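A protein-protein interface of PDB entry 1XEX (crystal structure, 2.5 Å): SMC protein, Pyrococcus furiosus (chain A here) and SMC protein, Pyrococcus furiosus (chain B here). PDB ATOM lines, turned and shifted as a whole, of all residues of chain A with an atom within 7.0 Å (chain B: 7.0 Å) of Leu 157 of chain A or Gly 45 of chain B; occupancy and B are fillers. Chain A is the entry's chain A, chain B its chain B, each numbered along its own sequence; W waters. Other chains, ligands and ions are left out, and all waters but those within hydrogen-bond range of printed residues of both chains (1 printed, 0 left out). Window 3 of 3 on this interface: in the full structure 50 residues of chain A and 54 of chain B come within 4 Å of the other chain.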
ATOM      1  N   MET A 154     -24.478  -1.951 -38.506  1.00  0.00           N
ATOM      2  CA  MET A 154     -24.743  -1.721 -37.087  1.00  0.00           C
ATOM      3  C   MET A 154     -25.734  -2.700 -36.475  1.00  0.00           C
ATOM      4  O   MET A 154     -26.714  -3.093 -37.104  1.00  0.00           O
ATOM      5  CB  MET A 154     -25.252  -0.292 -36.857  1.00  0.00           C
ATOM      6  CG  MET A 154     -24.159   0.769 -36.814  1.00  0.00           C
ATOM      7  SD  MET A 154     -24.807   2.469 -36.779  1.00  0.00           S
ATOM      8  CE  MET A 154     -25.381   2.592 -35.106  1.00  0.00           C
ATOM      9  N   SER A 155     -25.457  -3.096 -35.237  1.00  0.00           N
ATOM     10  CA  SER A 155     -26.326  -4.003 -34.496  1.00  0.00           C
ATOM     11  C   SER A 155     -27.290  -3.117 -33.707  1.00  0.00           C
ATOM     12  O   SER A 155     -26.965  -1.965 -33.395  1.00  0.00           O
ATOM     13  CB  SER A 155     -25.503  -4.859 -33.530  1.00  0.00           C
ATOM     14  OG  SER A 155     -24.922  -4.065 -32.503  1.00  0.00           O
ATOM     15  N   PRO A 156     -28.487  -3.636 -33.375  1.00  0.00           N
ATOM     16  CA  PRO A 156     -29.486  -2.867 -32.621  1.00  0.00           C
ATOM     17  C   PRO A 156     -28.888  -2.169 -31.404  1.00  0.00           C
ATOM     18  O   PRO A 156     -29.432  -1.180 -30.910  1.00  0.00           O
ATOM     19  CB  PRO A 156     -30.513  -3.923 -32.247  1.00  0.00           C
ATOM     20  CG  PRO A 156     -30.469  -4.837 -33.437  1.00  0.00           C
ATOM     21  CD  PRO A 156     -28.985  -4.990 -33.672  1.00  0.00           C
ATOM     22  N   LEU A 157     -27.763  -2.696 -30.933  1.00  0.00           N
ATOM     23  CA  LEU A 157     -27.055  -2.139 -29.785  1.00  0.00           C
ATOM     24  C   LEU A 157     -26.412  -0.819 -30.182  1.00  0.00           C
ATOM     25  O   LEU A 157     -26.799   0.248 -29.698  1.00  0.00           O
ATOM     26  CB  LEU A 157     -25.973  -3.111 -29.317  1.00  0.00           C
ATOM     27  CG  LEU A 157     -26.483  -4.462 -28.816  1.00  0.00           C
ATOM     28  CD1 LEU A 157     -25.296  -5.396 -28.539  1.00  0.00           C
ATOM     29  CD2 LEU A 157     -27.343  -4.242 -27.555  1.00  0.00           C
ATOM     30  N   GLU A 158     -25.427  -0.911 -31.072  1.00  0.00           N
ATOM     31  CA  GLU A 158     -24.701   0.251 -31.565  1.00  0.00           C
ATOM     32  C   GLU A 158     -25.690   1.339 -31.980  1.00  0.00           C
ATOM     33  O   GLU A 158     -25.437   2.533 -31.814  1.00  0.00           O
ATOM     34  CB  GLU A 158     -23.849  -0.161 -32.764  1.00  0.00           C
ATOM     35  CG  GLU A 158     -23.385  -1.603 -32.695  1.00  0.00           C
ATOM     36  CD  GLU A 158     -22.533  -2.011 -33.880  1.00  0.00           C
ATOM     37  OE1 GLU A 158     -21.433  -1.445 -34.043  1.00  0.00           O
ATOM     38  OE2 GLU A 158     -22.957  -2.899 -34.651  1.00  0.00           O
ATOM     39  N   ARG A 159     -26.830   0.908 -32.505  1.00  0.00           N
ATOM     40  CA  ARG A 159     -27.880   1.810 -32.967  1.00  0.00           C
ATOM     41  C   ARG A 159     -28.557   2.529 -31.804  1.00  0.00           C
ATOM     42  O   ARG A 159     -28.918   3.703 -31.901  1.00  0.00           O
ATOM     43  CB  ARG A 159     -28.901   1.000 -33.761  1.00  0.00           C
ATOM     44  CG  ARG A 159     -29.912   1.793 -34.552  1.00  0.00           C
ATOM     45  CD  ARG A 159     -30.697   0.830 -35.430  1.00  0.00           C
ATOM     46  NE  ARG A 159     -29.795   0.040 -36.265  1.00  0.00           N
ATOM     47  CZ  ARG A 159     -30.032  -1.205 -36.668  1.00  0.00           C
ATOM     48  NH1 ARG A 159     -31.155  -1.823 -36.314  1.00  0.00           N
ATOM     49  NH2 ARG A 159     -29.140  -1.835 -37.423  1.00  0.00           N
ATOM     50  N   ARG A 160     -28.732   1.820 -30.697  1.00  0.00           N
ATOM     51  CA  ARG A 160     -29.366   2.422 -29.535  1.00  0.00           C
ATOM     52  C   ARG A 160     -28.371   3.417 -28.954  1.00  0.00           C
ATOM     53  O   ARG A 160     -28.742   4.507 -28.507  1.00  0.00           O
ATOM     54  CB  ARG A 160     -29.718   1.342 -28.503  1.00  0.00           C
ATOM     55  CG  ARG A 160     -30.767   1.761 -27.472  1.00  0.00           C
ATOM     56  CD  ARG A 160     -30.241   2.794 -26.486  1.00  0.00           C
ATOM     57  NE  ARG A 160     -29.036   2.328 -25.804  1.00  0.00           N
ATOM     58  CZ  ARG A 160     -28.980   1.265 -25.006  1.00  0.00           C
ATOM     59  NH1 ARG A 160     -30.069   0.538 -24.769  1.00  0.00           N
ATOM     60  NH2 ARG A 160     -27.824   0.930 -24.451  1.00  0.00           N
ATOM     61  N   LEU A 161     -27.096   3.044 -28.985  1.00  0.00           N
ATOM     62  CA  LEU A 161     -26.047   3.901 -28.459  1.00  0.00           C
ATOM     63  C   LEU A 161     -25.914   5.218 -29.232  1.00  0.00           C
ATOM     64  O   LEU A 161     -25.552   6.248 -28.657  1.00  0.00           O
ATOM     65  CB  LEU A 161     -24.717   3.138 -28.455  1.00  0.00           C
ATOM     66  CG  LEU A 161     -24.719   1.878 -27.580  1.00  0.00           C
ATOM     67  CD1 LEU A 161     -23.364   1.184 -27.670  1.00  0.00           C
ATOM     68  CD2 LEU A 161     -25.051   2.251 -26.130  1.00  0.00           C
ATOM     69  N   LEU A 162     -26.210   5.194 -30.530  1.00  0.00           N
ATOM     70  CA  LEU A 162     -26.114   6.410 -31.330  1.00  0.00           C
ATOM     71  C   LEU A 162     -27.068   7.475 -30.834  1.00  0.00           C
ATOM     72  O   LEU A 162     -26.694   8.643 -30.721  1.00  0.00           O
ATOM     73  CB  LEU A 162     -26.409   6.129 -32.798  1.00  0.00           C
ATOM     74  CG  LEU A 162     -25.189   6.255 -33.704  1.00  0.00           C
ATOM     75  CD1 LEU A 162     -24.118   5.255 -33.253  1.00  0.00           C
ATOM     76  CD2 LEU A 162     -25.606   6.011 -35.149  1.00  0.00           C
ATOM     77  N   ASP A 164     -27.928   7.732 -28.043  1.00  0.00           N
ATOM     78  CA  ASP A 164     -27.427   8.105 -26.723  1.00  0.00           C
ATOM     79  C   ASP A 164     -26.675   9.417 -26.880  1.00  0.00           C
ATOM     80  O   ASP A 164     -26.900  10.372 -26.133  1.00  0.00           O
ATOM     81  CB  ASP A 164     -26.472   7.044 -26.154  1.00  0.00           C
ATOM     82  CG  ASP A 164     -27.195   5.952 -25.372  1.00  0.00           C
ATOM     83  OD1 ASP A 164     -28.114   6.288 -24.595  1.00  0.00           O
ATOM     84  OD2 ASP A 164     -26.833   4.761 -25.519  1.00  0.00           O
ATOM     85  N   GLU B  37     -36.609  -2.185 -27.933  1.00  0.00           N
ATOM     86  CA  GLU B  37     -36.577  -3.558 -27.434  1.00  0.00           C
ATOM     87  C   GLU B  37     -36.912  -3.628 -25.940  1.00  0.00           C
ATOM     88  O   GLU B  37     -37.522  -4.593 -25.477  1.00  0.00           O
ATOM     89  CB  GLU B  37     -35.196  -4.173 -27.696  1.00  0.00           C
ATOM     90  CG  GLU B  37     -35.086  -5.663 -27.386  1.00  0.00           C
ATOM     91  CD  GLU B  37     -33.751  -6.255 -27.811  1.00  0.00           C
ATOM     92  OE1 GLU B  37     -33.741  -7.136 -28.695  1.00  0.00           O
ATOM     93  OE2 GLU B  37     -32.710  -5.841 -27.256  1.00  0.00           O
ATOM     94  N   ASN B  38     -36.549  -2.582 -25.202  1.00  0.00           N
ATOM     95  CA  ASN B  38     -36.791  -2.529 -23.762  1.00  0.00           C
ATOM     96  C   ASN B  38     -37.372  -1.186 -23.310  1.00  0.00           C
ATOM     97  O   ASN B  38     -36.652  -0.333 -22.799  1.00  0.00           O
ATOM     98  CB  ASN B  38     -35.480  -2.816 -23.015  1.00  0.00           C
ATOM     99  CG  ASN B  38     -35.571  -2.524 -21.528  1.00  0.00           C
ATOM    100  OD1 ASN B  38     -36.501  -2.974 -20.845  1.00  0.00           O
ATOM    101  ND2 ASN B  38     -34.591  -1.779 -21.008  1.00  0.00           N
ATOM    102  N   PHE B  43     -33.842   0.907 -21.520  1.00  0.00           N
ATOM    103  CA  PHE B  43     -32.719   1.085 -22.433  1.00  0.00           C
ATOM    104  C   PHE B  43     -31.579   0.131 -22.060  1.00  0.00           C
ATOM    105  O   PHE B  43     -30.408   0.516 -22.024  1.00  0.00           O
ATOM    106  CB  PHE B  43     -32.247   2.540 -22.378  1.00  0.00           C
ATOM    107  CG  PHE B  43     -32.053   3.050 -20.983  1.00  0.00           C
ATOM    108  CD1 PHE B  43     -30.849   2.839 -20.309  1.00  0.00           C
ATOM    109  CD2 PHE B  43     -33.100   3.687 -20.312  1.00  0.00           C
ATOM    110  CE1 PHE B  43     -30.683   3.255 -18.974  1.00  0.00           C
ATOM    111  CE2 PHE B  43     -32.957   4.110 -18.973  1.00  0.00           C
ATOM    112  CZ  PHE B  43     -31.740   3.891 -18.302  1.00  0.00           C
ATOM    113  N   SER B  44     -31.935  -1.117 -21.767  1.00  0.00           N
ATOM    114  CA  SER B  44     -30.946  -2.127 -21.405  1.00  0.00           C
ATOM    115  C   SER B  44     -30.483  -2.865 -22.656  1.00  0.00           C
ATOM    116  O   SER B  44     -29.338  -3.327 -22.728  1.00  0.00           O
ATOM    117  CB  SER B  44     -31.536  -3.138 -20.417  1.00  0.00           C
ATOM    118  OG  SER B  44     -32.024  -2.494 -19.252  1.00  0.00           O
ATOM    119  N   GLY B  45     -31.384  -2.968 -23.636  1.00  0.00           N
ATOM    120  CA  GLY B  45     -31.070  -3.655 -24.876  1.00  0.00           C
ATOM    121  C   GLY B  45     -30.638  -2.736 -26.010  1.00  0.00           C
ATOM    122  O   GLY B  45     -29.631  -2.031 -25.894  1.00  0.00           O
ATOM    123  N   GLY B  46     -31.383  -2.743 -27.113  1.00  0.00           N
ATOM    124  CA  GLY B  46     -31.024  -1.892 -28.239  1.00  0.00           C
ATOM    125  C   GLY B  46     -32.192  -1.217 -28.948  1.00  0.00           C
ATOM    126  O   GLY B  46     -33.321  -1.162 -28.428  1.00  0.00           O
ATOM    127  N   LEU B  47     -31.918  -0.685 -30.137  1.00  0.00           N
ATOM    128  CA  LEU B  47     -32.946  -0.026 -30.931  1.00  0.00           C
ATOM    129  C   LEU B  47     -33.115  -0.865 -32.196  1.00  0.00           C
ATOM    130  O   LEU B  47     -32.150  -1.117 -32.918  1.00  0.00           O
ATOM    131  CB  LEU B  47     -32.511   1.402 -31.276  1.00  0.00           C
ATOM    132  CG  LEU B  47     -33.615   2.414 -31.608  1.00  0.00           C
ATOM    133  CD1 LEU B  47     -33.005   3.808 -31.752  1.00  0.00           C
ATOM    134  CD2 LEU B  47     -34.344   1.999 -32.879  1.00  0.00           C
ATOM    135  N   GLU B  48     -34.340  -1.320 -32.438  1.00  0.00           N
ATOM    136  CA  GLU B  48     -34.640  -2.147 -33.602  1.00  0.00           C
ATOM    137  C   GLU B  48     -35.395  -1.323 -34.637  1.00  0.00           C
ATOM    138  O   GLU B  48     -36.011  -0.308 -34.304  1.00  0.00           O
ATOM    139  CB  GLU B  48     -35.497  -3.349 -33.189  1.00  0.00           C
ATOM    140  CG  GLU B  48     -34.926  -4.162 -32.036  1.00  0.00           C
ATOM    141  CD  GLU B  48     -33.912  -5.207 -32.475  1.00  0.00           C
ATOM    142  OE1 GLU B  48     -33.298  -5.849 -31.586  1.00  0.00           O
ATOM    143  OE2 GLU B  48     -33.728  -5.402 -33.702  1.00  0.00           O
HETATM  144  O   HOH W   1     -33.287  -3.588 -36.165  1.00  0.00           O
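The backbone carbonyl oxygen (O) of Met 154 of chain A lies within hydrogen-bond range of the guanidinium group (NH2) of Arg 159 of chain A.
The side-chain amide nitrogen of Asn 38 of chain B sits close to the backbone NH of Phe 43 of chain B, at 2.8 Å.
The backbone NH (N) of Ser 44 of chain B sits close to the side-chain amide nitrogen (ND2) of Asn 38 of chain B (2.8 Å).
The side-chain carboxylate of Asp 164 of chain A lies within salt-bridge range of the guanidinium group of Arg 160 of chain A, 3.3 Å away.
The backbone NH of Gly 46 of chain B lies within hydrogen-bond range of the side-chain carboxylate of Glu 37 of chain B, 3.4 Å away.
Gly 45 of chain B touches two residues of chain A.
Printed residues of chain A within 4 Å of Phe 43 of chain B: Arg 160.
Printed residues of chain B within 4 Å of Arg 160 of chain A: Phe 43 (2.8 Å), Ser 44 (3.9 Å), Gly 45 (2.8 Å), Gly 46 (3.5 Å) and Leu 47 (3.4 Å).
Of the printed residues of chain A, Gly 46 of chain B touches Pro 156 (3.2 Å) and Arg 160 (3.5 Å).
Met 154 of chain A touches none of the printed residues of chain B.
The nearest printed residue of chain B that does not touch Pro 156 of chain A is Gly 45 of chain B (5.1 Å).
Water W1 bridges the guanidinium group of Arg 159 of chain A (2.8 Å) and the side-chain carboxylate of Glu 48 of chain B (3.1 Å).
Of the 8 printed residues of chain B, 6 touch a printed residue of chain A.
Hydrophobic or aromatic side chains of chain B within 4 Å of the printed part of chain A: Phe 43 and Leu 47.
Hydrophobic or aromatic side chains of chain A within 4 Å of the printed part of chain B: Pro 156 and Leu 157.
Among the printed residues, 10 pairs touch across the chains.
Among the printed residues, no Asp or Glu carboxylate lies within 4 Å of a Lys or Arg side-chain nitrogen of the other chain.
NH1 of Arg 160 of chain A is in hydrogen-bond range of O of Gly 45 of chain B.
The backbone carbonyl oxygen (O) of Pro 156 of chain A is in hydrogen-bond range of the backbone NH (N) of Leu 47 of chain B (2.7 Å).
NH1 of Arg 160 of chain A lies within hydrogen-bond range of O of Phe 43 of chain B (2.8 Å).
Gly 46 of chain B touches Pro 156 of chain A.
Pro 156 of chain A touches Glu 48 of chain B.
Leu 157 of chain A touches Gly 45 of chain B.
Arg 159 of chain A touches Leu 47 of chain B (CD to O, 3.5 Å).
Arg 160 of chain A touches Ser 44 of chain B (NH1 to N, 3.9 Å).
Arg 160 of chain A touches Gly 46 of chain B.
CB of Arg 160 of chain A touches N of Leu 47 of chain B, at 3.4 Å.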
